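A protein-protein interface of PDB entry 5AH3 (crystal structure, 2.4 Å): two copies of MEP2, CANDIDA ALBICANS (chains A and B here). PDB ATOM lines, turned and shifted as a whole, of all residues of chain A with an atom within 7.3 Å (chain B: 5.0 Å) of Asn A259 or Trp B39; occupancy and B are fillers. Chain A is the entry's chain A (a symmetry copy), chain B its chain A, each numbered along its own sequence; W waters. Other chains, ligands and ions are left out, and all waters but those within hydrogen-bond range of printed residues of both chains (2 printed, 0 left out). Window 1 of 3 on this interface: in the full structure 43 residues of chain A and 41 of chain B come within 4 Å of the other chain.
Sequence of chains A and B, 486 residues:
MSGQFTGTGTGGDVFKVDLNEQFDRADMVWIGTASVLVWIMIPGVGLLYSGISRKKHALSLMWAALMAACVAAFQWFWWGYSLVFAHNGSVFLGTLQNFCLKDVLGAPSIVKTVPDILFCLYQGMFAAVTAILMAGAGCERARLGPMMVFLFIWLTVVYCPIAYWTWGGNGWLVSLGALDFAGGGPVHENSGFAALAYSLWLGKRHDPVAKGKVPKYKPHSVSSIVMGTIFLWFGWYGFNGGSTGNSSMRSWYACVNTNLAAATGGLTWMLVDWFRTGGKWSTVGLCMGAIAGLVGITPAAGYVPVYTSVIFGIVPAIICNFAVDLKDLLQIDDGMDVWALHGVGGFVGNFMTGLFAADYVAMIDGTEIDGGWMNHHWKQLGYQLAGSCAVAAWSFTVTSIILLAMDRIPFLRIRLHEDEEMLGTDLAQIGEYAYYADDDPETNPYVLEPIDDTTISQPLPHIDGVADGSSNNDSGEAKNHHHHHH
The indole nitrogen (NE1) of Trp A233 lies within hydrogen-bond range of the side-chain amide oxygen (OD1) of Asn A259 (3.4 Å).
The side-chain hydroxyl (OG1) of Thr A264 is in hydrogen-bond range of the backbone carbonyl oxygen (O) of Leu A260 (2.9 Å).
NE1 of Trp A233 lies within hydrogen-bond range of OH of Tyr A237 (3.4 Å).
The side-chain amide oxygen (OD1) of Asn A259 is in hydrogen-bond range of the side-chain hydroxyl (OH) of Tyr A237, 3.2 Å away.
Leu B66 touches Thr A229 (CD1 to CG2, 3.9 Å).
O of Ile A230 touches CZ3 of Trp B39 (3.8 Å).
Ile A230 touches Pro B43 (CD1 to CB, 3.5 Å).
Trp A233 touches Trp B39.
Val B36 touches Phe A234 (O to CE1, 3.4 Å).
CD1 of Phe A234 touches CB of Ile B40, at 3.8 Å.
CG2 of Val B36 touches CB of Tyr A237, 3.6 Å away.
OH of Tyr A237 touches CD1 of Trp B39, 3.3 Å away.
OH of Tyr A237 touches CE of Met B125 (3.5 Å).
OD1 of Asn A259 touches NE1 of Trp B39, at 3.9 Å.
Printed residues of chain B within 4 Å of Phe A234: Val B36 and Ile B40.
Of chain B, only Trp B39 and Ala B73 come within 4 Å of Asn A259.
Of the printed residues of chain A, Val B36 touches Phe A234 (3.4 Å) and Tyr A237 (3.6 Å).
Of chain A, only Ile A230 (3.8 Å), Trp A233 (3.2 Å), Tyr A237 (3.3 Å) and Asn A259 (3.9 Å) come within 4 Å of Trp B39.
The nearest residue of chain A that does not touch Trp B39 is Phe A234 (4.1 Å).
The nearest printed residue of chain A that does not touch Pro B43 is Phe A231 (7.3 Å).
Of the 13 printed residues of chain B, 7 touch a printed residue of chain A.
Hydrophobic or aromatic side chains of chain A that line the printed part of chain B: Ile A230, Trp A233, Phe A234, Tyr A237, Leu A260 and Ala A263.
Among the printed residues, no Asp or Glu carboxylate lies within 4 Å of a Lys or Arg side-chain nitrogen of the other chain.
No position is printed for both chains.
Of the 13 pairs that touch across the chains among the printed residues, none has its exchanged pair printed and touching as well.
Water W1 lies within hydrogen-bond range of O of Ala B69 (2.9 Å), OD1 of Asn A259 (3.1 Å) and NE1 of Trp B39 (3.1 Å).
Water W2 bridges the side-chain amide nitrogen of Asn A259 and the side-chain sulfur of Met B125.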
ATOM      1  N   THR A 229      -1.173  22.653 -16.990  1.00  0.00           N
ATOM      2  CA  THR A 229      -1.318  22.126 -18.338  1.00  0.00           C
ATOM      3  C   THR A 229      -1.291  20.587 -18.347  1.00  0.00           C
ATOM      4  O   THR A 229      -1.973  19.952 -19.155  1.00  0.00           O
ATOM      5  CB  THR A 229      -0.202  22.692 -19.262  1.00  0.00           C
ATOM      6  OG1 THR A 229      -0.237  24.122 -19.210  1.00  0.00           O
ATOM      7  CG2 THR A 229      -0.383  22.241 -20.707  1.00  0.00           C
ATOM      8  N   ILE A 230      -0.497  20.000 -17.453  1.00  0.00           N
ATOM      9  CA  ILE A 230      -0.391  18.556 -17.361  1.00  0.00           C
ATOM     10  C   ILE A 230      -1.718  17.957 -16.888  1.00  0.00           C
ATOM     11  O   ILE A 230      -2.230  17.025 -17.496  1.00  0.00           O
ATOM     12  CB  ILE A 230       0.742  18.129 -16.408  1.00  0.00           C
ATOM     13  CG1 ILE A 230       2.113  18.398 -17.033  1.00  0.00           C
ATOM     14  CG2 ILE A 230       0.639  16.639 -16.046  1.00  0.00           C
ATOM     15  CD1 ILE A 230       3.273  18.350 -16.020  1.00  0.00           C
ATOM     16  N   PHE A 231      -2.263  18.502 -15.799  1.00  0.00           N
ATOM     17  CA  PHE A 231      -3.525  18.031 -15.247  1.00  0.00           C
ATOM     18  C   PHE A 231      -4.687  18.180 -16.233  1.00  0.00           C
ATOM     19  O   PHE A 231      -5.582  17.332 -16.286  1.00  0.00           O
ATOM     20  CB  PHE A 231      -3.866  18.779 -13.957  1.00  0.00           C
ATOM     21  CG  PHE A 231      -3.097  18.299 -12.743  1.00  0.00           C
ATOM     22  CD1 PHE A 231      -2.320  17.161 -12.798  1.00  0.00           C
ATOM     23  CD2 PHE A 231      -3.167  18.987 -11.545  1.00  0.00           C
ATOM     24  CE1 PHE A 231      -1.620  16.727 -11.685  1.00  0.00           C
ATOM     25  CE2 PHE A 231      -2.472  18.548 -10.427  1.00  0.00           C
ATOM     26  CZ  PHE A 231      -1.698  17.423 -10.501  1.00  0.00           C
ATOM     27  N   LEU A 232      -4.662  19.277 -16.984  1.00  0.00           N
ATOM     28  CA  LEU A 232      -5.718  19.630 -17.919  1.00  0.00           C
ATOM     29  C   LEU A 232      -5.722  18.730 -19.148  1.00  0.00           C
ATOM     30  O   LEU A 232      -6.774  18.331 -19.609  1.00  0.00           O
ATOM     31  CB  LEU A 232      -5.581  21.098 -18.346  1.00  0.00           C
ATOM     32  CG  LEU A 232      -6.133  22.131 -17.348  1.00  0.00           C
ATOM     33  CD1 LEU A 232      -5.592  23.519 -17.629  1.00  0.00           C
ATOM     34  CD2 LEU A 232      -7.660  22.137 -17.384  1.00  0.00           C
ATOM     35  N   TRP A 233      -4.539  18.426 -19.668  1.00  0.00           N
ATOM     36  CA  TRP A 233      -4.398  17.588 -20.842  1.00  0.00           C
ATOM     37  C   TRP A 233      -4.752  16.127 -20.477  1.00  0.00           C
ATOM     38  O   TRP A 233      -5.504  15.476 -21.184  1.00  0.00           O
ATOM     39  CB  TRP A 233      -2.980  17.739 -21.391  1.00  0.00           C
ATOM     40  CG  TRP A 233      -2.661  17.113 -22.726  1.00  0.00           C
ATOM     41  CD1 TRP A 233      -3.248  16.014 -23.300  1.00  0.00           C
ATOM     42  CD2 TRP A 233      -1.630  17.535 -23.638  1.00  0.00           C
ATOM     43  NE1 TRP A 233      -2.651  15.740 -24.509  1.00  0.00           N
ATOM     44  CE2 TRP A 233      -1.658  16.654 -24.740  1.00  0.00           C
ATOM     45  CE3 TRP A 233      -0.687  18.582 -23.627  1.00  0.00           C
ATOM     46  CZ2 TRP A 233      -0.787  16.787 -25.825  1.00  0.00           C
ATOM     47  CZ3 TRP A 233       0.178  18.711 -24.700  1.00  0.00           C
ATOM     48  CH2 TRP A 233       0.127  17.817 -25.784  1.00  0.00           C
ATOM     49  N   PHE A 234      -4.234  15.659 -19.342  1.00  0.00           N
ATOM     50  CA  PHE A 234      -4.589  14.383 -18.734  1.00  0.00           C
ATOM     51  C   PHE A 234      -6.114  14.195 -18.527  1.00  0.00           C
ATOM     52  O   PHE A 234      -6.693  13.187 -18.951  1.00  0.00           O
ATOM     53  CB  PHE A 234      -3.857  14.263 -17.406  1.00  0.00           C
ATOM     54  CG  PHE A 234      -4.069  12.970 -16.663  1.00  0.00           C
ATOM     55  CD1 PHE A 234      -3.509  11.776 -17.113  1.00  0.00           C
ATOM     56  CD2 PHE A 234      -4.738  12.966 -15.454  1.00  0.00           C
ATOM     57  CE1 PHE A 234      -3.658  10.616 -16.387  1.00  0.00           C
ATOM     58  CE2 PHE A 234      -4.887  11.810 -14.719  1.00  0.00           C
ATOM     59  CZ  PHE A 234      -4.350  10.635 -15.188  1.00  0.00           C
ATOM     60  N   GLY A 235      -6.752  15.164 -17.881  1.00  0.00           N
ATOM     61  CA  GLY A 235      -8.180  15.123 -17.648  1.00  0.00           C
ATOM     62  C   GLY A 235      -9.057  15.262 -18.885  1.00  0.00           C
ATOM     63  O   GLY A 235     -10.191  14.770 -18.909  1.00  0.00           O
ATOM     64  N   TYR A 237      -9.039  13.850 -21.588  1.00  0.00           N
ATOM     65  CA  TYR A 237      -9.378  12.580 -22.203  1.00  0.00           C
ATOM     66  C   TYR A 237     -10.758  12.110 -21.731  1.00  0.00           C
ATOM     67  O   TYR A 237     -11.507  11.560 -22.516  1.00  0.00           O
ATOM     68  CB  TYR A 237      -8.311  11.530 -21.908  1.00  0.00           C
ATOM     69  CG  TYR A 237      -7.008  11.779 -22.647  1.00  0.00           C
ATOM     70  CD1 TYR A 237      -6.942  11.713 -24.041  1.00  0.00           C
ATOM     71  CD2 TYR A 237      -5.833  12.063 -21.948  1.00  0.00           C
ATOM     72  CE1 TYR A 237      -5.730  11.948 -24.713  1.00  0.00           C
ATOM     73  CE2 TYR A 237      -4.631  12.283 -22.605  1.00  0.00           C
ATOM     74  CZ  TYR A 237      -4.577  12.238 -23.976  1.00  0.00           C
ATOM     75  OH  TYR A 237      -3.359  12.456 -24.601  1.00  0.00           O
ATOM     76  N   ASN A 240     -13.474  15.067 -23.117  1.00  0.00           N
ATOM     77  CA  ASN A 240     -13.895  14.833 -24.491  1.00  0.00           C
ATOM     78  C   ASN A 240     -14.304  13.356 -24.756  1.00  0.00           C
ATOM     79  O   ASN A 240     -15.369  13.098 -25.296  1.00  0.00           O
ATOM     80  CB  ASN A 240     -12.785  15.272 -25.457  1.00  0.00           C
ATOM     81  CG  ASN A 240     -12.789  16.781 -25.717  1.00  0.00           C
ATOM     82  OD1 ASN A 240     -13.618  17.513 -25.181  1.00  0.00           O
ATOM     83  ND2 ASN A 240     -11.856  17.245 -26.549  1.00  0.00           N
ATOM     84  N   ALA A 254     -12.271  10.164 -30.504  1.00  0.00           N
ATOM     85  CA  ALA A 254     -12.360  11.502 -29.961  1.00  0.00           C
ATOM     86  C   ALA A 254     -11.120  11.842 -29.103  1.00  0.00           C
ATOM     87  O   ALA A 254     -10.743  12.991 -29.011  1.00  0.00           O
ATOM     88  CB  ALA A 254     -13.639  11.656 -29.135  1.00  0.00           C
ATOM     89  N   CYS A 255     -10.509  10.821 -28.497  1.00  0.00           N
ATOM     90  CA  CYS A 255      -9.307  10.962 -27.699  1.00  0.00           C
ATOM     91  C   CYS A 255      -8.083  11.248 -28.568  1.00  0.00           C
ATOM     92  O   CYS A 255      -7.232  12.069 -28.208  1.00  0.00           O
ATOM     93  CB  CYS A 255      -9.052   9.710 -26.865  1.00  0.00           C
ATOM     94  SG  CYS A 255     -10.009   9.554 -25.379  1.00  0.00           S
ATOM     95  N   VAL A 256      -7.999  10.556 -29.700  1.00  0.00           N
ATOM     96  CA  VAL A 256      -6.965  10.800 -30.691  1.00  0.00           C
ATOM     97  C   VAL A 256      -7.047  12.249 -31.201  1.00  0.00           C
ATOM     98  O   VAL A 256      -6.021  12.937 -31.301  1.00  0.00           O
ATOM     99  CB  VAL A 256      -7.073   9.799 -31.868  1.00  0.00           C
ATOM    100  CG1 VAL A 256      -6.199  10.210 -33.029  1.00  0.00           C
ATOM    101  CG2 VAL A 256      -6.703   8.391 -31.402  1.00  0.00           C
ATOM    102  N   ASN A 257      -8.266  12.710 -31.500  1.00  0.00           N
ATOM    103  CA  ASN A 257      -8.491  14.092 -31.921  1.00  0.00           C
ATOM    104  C   ASN A 257      -8.042  15.124 -30.859  1.00  0.00           C
ATOM    105  O   ASN A 257      -7.538  16.184 -31.200  1.00  0.00           O
ATOM    106  CB  ASN A 257      -9.973  14.319 -32.262  1.00  0.00           C
ATOM    107  CG  ASN A 257     -10.345  13.860 -33.683  1.00  0.00           C
ATOM    108  OD1 ASN A 257      -9.493  13.746 -34.561  1.00  0.00           O
ATOM    109  ND2 ASN A 257     -11.643  13.616 -33.907  1.00  0.00           N
ATOM    110  N   THR A 258      -8.267  14.793 -29.588  1.00  0.00           N
ATOM    111  CA  THR A 258      -7.936  15.621 -28.439  1.00  0.00           C
ATOM    112  C   THR A 258      -6.409  15.787 -28.272  1.00  0.00           C
ATOM    113  O   THR A 258      -5.895  16.898 -28.148  1.00  0.00           O
ATOM    114  CB  THR A 258      -8.559  15.015 -27.150  1.00  0.00           C
ATOM    115  OG1 THR A 258      -9.994  15.091 -27.216  1.00  0.00           O
ATOM    116  CG2 THR A 258      -8.072  15.750 -25.895  1.00  0.00           C
ATOM    117  N   ASN A 259      -5.706  14.661 -28.295  1.00  0.00           N
ATOM    118  CA  ASN A 259      -4.261  14.613 -28.290  1.00  0.00           C
ATOM    119  C   ASN A 259      -3.642  15.420 -29.439  1.00  0.00           C
ATOM    120  O   ASN A 259      -2.754  16.245 -29.221  1.00  0.00           O
ATOM    121  CB  ASN A 259      -3.810  13.150 -28.351  1.00  0.00           C
ATOM    122  CG  ASN A 259      -2.360  12.967 -27.962  1.00  0.00           C
ATOM    123  OD1 ASN A 259      -1.836  13.675 -27.093  1.00  0.00           O
ATOM    124  ND2 ASN A 259      -1.703  12.012 -28.601  1.00  0.00           N
ATOM    125  N   LEU A 260      -4.129  15.211 -30.659  1.00  0.00           N
ATOM    126  CA  LEU A 260      -3.535  15.860 -31.827  1.00  0.00           C
ATOM    127  C   LEU A 260      -3.776  17.379 -31.896  1.00  0.00           C
ATOM    128  O   LEU A 260      -2.922  18.130 -32.373  1.00  0.00           O
ATOM    129  CB  LEU A 260      -4.059  15.207 -33.096  1.00  0.00           C
ATOM    130  CG  LEU A 260      -3.306  15.398 -34.408  1.00  0.00           C
ATOM    131  CD1 LEU A 260      -1.808  15.109 -34.239  1.00  0.00           C
ATOM    132  CD2 LEU A 260      -3.935  14.486 -35.496  1.00  0.00           C
ATOM    133  N   ALA A 261      -4.950  17.821 -31.447  1.00  0.00           N
ATOM    134  CA  ALA A 261      -5.269  19.245 -31.440  1.00  0.00           C
ATOM    135  C   ALA A 261      -4.411  20.000 -30.406  1.00  0.00           C
ATOM    136  O   ALA A 261      -3.966  21.103 -30.655  1.00  0.00           O
ATOM    137  CB  ALA A 261      -6.747  19.458 -31.162  1.00  0.00           C
ATOM    138  N   ALA A 262      -4.198  19.388 -29.254  1.00  0.00           N
ATOM    139  CA  ALA A 262      -3.344  19.929 -28.218  1.00  0.00           C
ATOM    140  C   ALA A 262      -1.921  20.074 -28.736  1.00  0.00           C
ATOM    141  O   ALA A 262      -1.312  21.135 -28.589  1.00  0.00           O
ATOM    142  CB  ALA A 262      -3.381  19.042 -26.974  1.00  0.00           C
ATOM    143  N   ALA A 263      -1.416  19.010 -29.359  1.00  0.00           N
ATOM    144  CA  ALA A 263      -0.042  18.960 -29.852  1.00  0.00           C
ATOM    145  C   ALA A 263       0.245  20.018 -30.913  1.00  0.00           C
ATOM    146  O   ALA A 263       1.277  20.707 -30.865  1.00  0.00           O
ATOM    147  CB  ALA A 263       0.273  17.576 -30.400  1.00  0.00           C
ATOM    148  N   THR A 264      -0.665  20.146 -31.871  1.00  0.00           N
ATOM    149  CA  THR A 264      -0.496  21.099 -32.966  1.00  0.00           C
ATOM    150  C   THR A 264      -0.771  22.524 -32.481  1.00  0.00           C
ATOM    151  O   THR A 264      -0.244  23.476 -33.030  1.00  0.00           O
ATOM    152  CB  THR A 264      -1.427  20.771 -34.175  1.00  0.00           C
ATOM    153  OG1 THR A 264      -2.786  20.718 -33.736  1.00  0.00           O
ATOM    154  CG2 THR A 264      -1.086  19.429 -34.779  1.00  0.00           C
ATOM    155  N   GLY A 265      -1.608  22.667 -31.460  1.00  0.00           N
ATOM    156  CA  GLY A 265      -1.841  23.971 -30.863  1.00  0.00           C
ATOM    157  C   GLY A 265      -0.585  24.474 -30.141  1.00  0.00           C
ATOM    158  O   GLY A 265      -0.203  25.631 -30.269  1.00  0.00           O
ATOM    159  N   LEU A 294      -7.030  22.207 -27.168  1.00  0.00           N
ATOM    160  CA  LEU A 294      -7.962  21.479 -26.330  1.00  0.00           C
ATOM    161  C   LEU A 294      -9.341  22.147 -26.327  1.00  0.00           C
ATOM    162  O   LEU A 294     -10.360  21.482 -26.524  1.00  0.00           O
ATOM    163  CB  LEU A 294      -7.395  21.367 -24.913  1.00  0.00           C
ATOM    164  CG  LEU A 294      -6.196  20.412 -24.831  1.00  0.00           C
ATOM    165  CD1 LEU A 294      -5.411  20.617 -23.555  1.00  0.00           C
ATOM    166  CD2 LEU A 294      -6.622  18.936 -24.959  1.00  0.00           C
ATOM    167  N   ILE A 297     -10.984  21.901 -29.991  1.00  0.00           N
ATOM    168  CA  ILE A 297     -11.458  20.604 -30.434  1.00  0.00           C
ATOM    169  C   ILE A 297     -12.653  20.112 -29.604  1.00  0.00           C
ATOM    170  O   ILE A 297     -13.286  19.140 -29.966  1.00  0.00           O
ATOM    171  CB  ILE A 297     -10.303  19.557 -30.392  1.00  0.00           C
ATOM    172  CG1 ILE A 297     -10.636  18.305 -31.209  1.00  0.00           C
ATOM    173  CG2 ILE A 297      -9.943  19.198 -28.954  1.00  0.00           C
ATOM    174  CD1 ILE A 297     -10.787  18.521 -32.685  1.00  0.00           C
ATOM    175  N   SER A 309      -8.359  17.485 -37.223  1.00  0.00           N
ATOM    176  CA  SER A 309      -8.160  17.848 -35.834  1.00  0.00           C
ATOM    177  C   SER A 309      -6.922  18.757 -35.697  1.00  0.00           C
ATOM    178  O   SER A 309      -6.825  19.540 -34.771  1.00  0.00           O
ATOM    179  CB  SER A 309      -8.024  16.601 -34.971  1.00  0.00           C
ATOM    180  OG  SER A 309      -6.861  15.875 -35.304  1.00  0.00           O
ATOM    181  N   SER B  35      -4.267   4.021 -21.826  1.00  0.00           N
ATOM    182  CA  SER B  35      -3.672   5.027 -22.707  1.00  0.00           C
ATOM    183  C   SER B  35      -3.501   6.371 -21.973  1.00  0.00           C
ATOM    184  O   SER B  35      -2.483   7.053 -22.102  1.00  0.00           O
ATOM    185  CB  SER B  35      -4.538   5.247 -23.958  1.00  0.00           C
ATOM    186  OG  SER B  35      -4.666   4.084 -24.762  1.00  0.00           O
ATOM    187  N   VAL B  36      -4.534   6.747 -21.237  1.00  0.00           N
ATOM    188  CA  VAL B  36      -4.523   7.960 -20.447  1.00  0.00           C
ATOM    189  C   VAL B  36      -3.430   7.889 -19.369  1.00  0.00           C
ATOM    190  O   VAL B  36      -2.686   8.853 -19.158  1.00  0.00           O
ATOM    191  CB  VAL B  36      -5.889   8.195 -19.810  1.00  0.00           C
ATOM    192  CG1 VAL B  36      -5.853   9.402 -18.909  1.00  0.00           C
ATOM    193  CG2 VAL B  36      -6.971   8.334 -20.906  1.00  0.00           C
ATOM    194  N   LEU B  37      -3.326   6.728 -18.726  1.00  0.00           N
ATOM    195  CA  LEU B  37      -2.323   6.497 -17.708  1.00  0.00           C
ATOM    196  C   LEU B  37      -0.906   6.618 -18.244  1.00  0.00           C
ATOM    197  O   LEU B  37      -0.062   7.247 -17.598  1.00  0.00           O
ATOM    198  CB  LEU B  37      -2.510   5.132 -17.062  1.00  0.00           C
ATOM    199  CG  LEU B  37      -3.762   5.004 -16.189  1.00  0.00           C
ATOM    200  CD1 LEU B  37      -3.970   3.555 -15.737  1.00  0.00           C
ATOM    201  CD2 LEU B  37      -3.712   5.960 -14.996  1.00  0.00           C
ATOM    202  N   VAL B  38      -0.641   6.027 -19.410  1.00  0.00           N
ATOM    203  CA  VAL B  38       0.698   6.088 -19.987  1.00  0.00           C
ATOM    204  C   VAL B  38       1.080   7.548 -20.306  1.00  0.00           C
ATOM    205  O   VAL B  38       2.235   7.921 -20.172  1.00  0.00           O
ATOM    206  CB  VAL B  38       0.837   5.210 -21.253  1.00  0.00           C
ATOM    207  CG1 VAL B  38       2.282   5.234 -21.789  1.00  0.00           C
ATOM    208  CG2 VAL B  38       0.452   3.773 -20.948  1.00  0.00           C
ATOM    209  N   TRP B  39       0.103   8.368 -20.685  1.00  0.00           N
ATOM    210  CA  TRP B  39       0.366   9.742 -21.058  1.00  0.00           C
ATOM    211  C   TRP B  39       1.019  10.552 -19.918  1.00  0.00           C
ATOM    212  O   TRP B  39       1.931  11.322 -20.166  1.00  0.00           O
ATOM    213  CB  TRP B  39      -0.910  10.459 -21.523  1.00  0.00           C
ATOM    214  CG  TRP B  39      -0.552  11.792 -22.152  1.00  0.00           C
ATOM    215  CD1 TRP B  39      -0.249  12.023 -23.468  1.00  0.00           C
ATOM    216  CD2 TRP B  39      -0.396  13.056 -21.483  1.00  0.00           C
ATOM    217  NE1 TRP B  39       0.068  13.354 -23.660  1.00  0.00           N
ATOM    218  CE2 TRP B  39      -0.011  14.005 -22.456  1.00  0.00           C
ATOM    219  CE3 TRP B  39      -0.534  13.473 -20.154  1.00  0.00           C
ATOM    220  CZ2 TRP B  39       0.236  15.347 -22.140  1.00  0.00           C
ATOM    221  CZ3 TRP B  39      -0.302  14.804 -19.842  1.00  0.00           C
ATOM    222  CH2 TRP B  39       0.078  15.727 -20.832  1.00  0.00           C
ATOM    223  N   ILE B  40       0.560  10.368 -18.684  1.00  0.00           N
ATOM    224  CA  ILE B  40       1.097  11.136 -17.577  1.00  0.00           C
ATOM    225  C   ILE B  40       2.501  10.651 -17.177  1.00  0.00           C
ATOM    226  O   ILE B  40       3.182  11.299 -16.378  1.00  0.00           O
ATOM    227  CB  ILE B  40       0.157  11.115 -16.348  1.00  0.00           C
ATOM    228  CG1 ILE B  40       0.368  12.403 -15.536  1.00  0.00           C
ATOM    229  CG2 ILE B  40       0.385   9.865 -15.515  1.00  0.00           C
ATOM    230  CD1 ILE B  40      -0.546  12.600 -14.386  1.00  0.00           C
ATOM    231  N   MET B  41       2.941   9.533 -17.751  1.00  0.00           N
ATOM    232  CA  MET B  41       4.318   9.090 -17.572  1.00  0.00           C
ATOM    233  C   MET B  41       5.293  10.031 -18.281  1.00  0.00           C
ATOM    234  O   MET B  41       6.483  10.037 -17.969  1.00  0.00           O
ATOM    235  CB  MET B  41       4.541   7.663 -18.096  1.00  0.00           C
ATOM    236  CG  MET B  41       3.817   6.564 -17.323  1.00  0.00           C
ATOM    237  SD  MET B  41       4.020   4.915 -18.031  1.00  0.00           S
ATOM    238  CE  MET B  41       5.733   4.553 -17.714  1.00  0.00           C
ATOM    239  N   ILE B  42       4.797  10.785 -19.258  1.00  0.00           N
ATOM    240  CA  ILE B  42       5.668  11.628 -20.061  1.00  0.00           C
ATOM    241  C   ILE B  42       6.231  12.801 -19.197  1.00  0.00           C
ATOM    242  O   ILE B  42       7.437  12.988 -19.139  1.00  0.00           O
ATOM    243  CB  ILE B  42       4.943  12.171 -21.323  1.00  0.00           C
ATOM    244  CG1 ILE B  42       4.395  11.029 -22.199  1.00  0.00           C
ATOM    245  CG2 ILE B  42       5.856  13.115 -22.120  1.00  0.00           C
ATOM    246  CD1 ILE B  42       3.281  11.505 -23.130  1.00  0.00           C
ATOM    247  N   PRO B  43       5.360  13.563 -18.506  1.00  0.00           N
ATOM    248  CA  PRO B  43       5.958  14.519 -17.573  1.00  0.00           C
ATOM    249  C   PRO B  43       6.669  13.848 -16.401  1.00  0.00           C
ATOM    250  O   PRO B  43       7.476  14.495 -15.732  1.00  0.00           O
ATOM    251  CB  PRO B  43       4.756  15.336 -17.080  1.00  0.00           C
ATOM    252  CG  PRO B  43       3.561  14.458 -17.333  1.00  0.00           C
ATOM    253  CD  PRO B  43       3.893  13.742 -18.597  1.00  0.00           C
ATOM    254  N   LEU B  66       6.312  18.410 -22.071  1.00  0.00           N
ATOM    255  CA  LEU B  66       5.170  18.867 -22.860  1.00  0.00           C
ATOM    256  C   LEU B  66       5.530  19.103 -24.331  1.00  0.00           C
ATOM    257  O   LEU B  66       4.722  18.825 -25.227  1.00  0.00           O
ATOM    258  CB  LEU B  66       4.573  20.134 -22.259  1.00  0.00           C
ATOM    259  CG  LEU B  66       3.845  19.959 -20.922  1.00  0.00           C
ATOM    260  CD1 LEU B  66       3.344  21.290 -20.435  1.00  0.00           C
ATOM    261  CD2 LEU B  66       2.677  18.960 -21.053  1.00  0.00           C
ATOM    262  N   ALA B  69       5.637  15.709 -25.920  1.00  0.00           N
ATOM    263  CA  ALA B  69       4.288  15.208 -26.125  1.00  0.00           C
ATOM    264  C   ALA B  69       3.706  15.763 -27.423  1.00  0.00           C
ATOM    265  O   ALA B  69       2.970  15.063 -28.128  1.00  0.00           O
ATOM    266  CB  ALA B  69       3.405  15.564 -24.936  1.00  0.00           C
ATOM    267  N   ALA B  73       3.266  13.277 -30.777  1.00  0.00           N
ATOM    268  CA  ALA B  73       1.894  13.065 -31.234  1.00  0.00           C
ATOM    269  C   ALA B  73       1.757  13.416 -32.705  1.00  0.00           C
ATOM    270  O   ALA B  73       1.032  12.732 -33.442  1.00  0.00           O
ATOM    271  CB  ALA B  73       0.910  13.864 -30.404  1.00  0.00           C
ATOM    272  N   MET B 125       1.293   6.683 -27.045  1.00  0.00           N
ATOM    273  CA  MET B 125       1.808   7.078 -25.740  1.00  0.00           C
ATOM    274  C   MET B 125       3.192   6.485 -25.471  1.00  0.00           C
ATOM    275  O   MET B 125       4.019   7.114 -24.800  1.00  0.00           O
ATOM    276  CB  MET B 125       0.863   6.654 -24.613  1.00  0.00           C
ATOM    277  CG  MET B 125      -0.575   7.092 -24.743  1.00  0.00           C
ATOM    278  SD  MET B 125      -0.773   8.827 -25.105  1.00  0.00           S
ATOM    279  CE  MET B 125      -2.550   9.030 -25.054  1.00  0.00           C
HETATM  280  O   HOH W   1       1.170  13.472 -26.541  1.00  0.00           O
HETATM  281  O   HOH W   2       1.130  10.701 -27.700  1.00  0.00           O
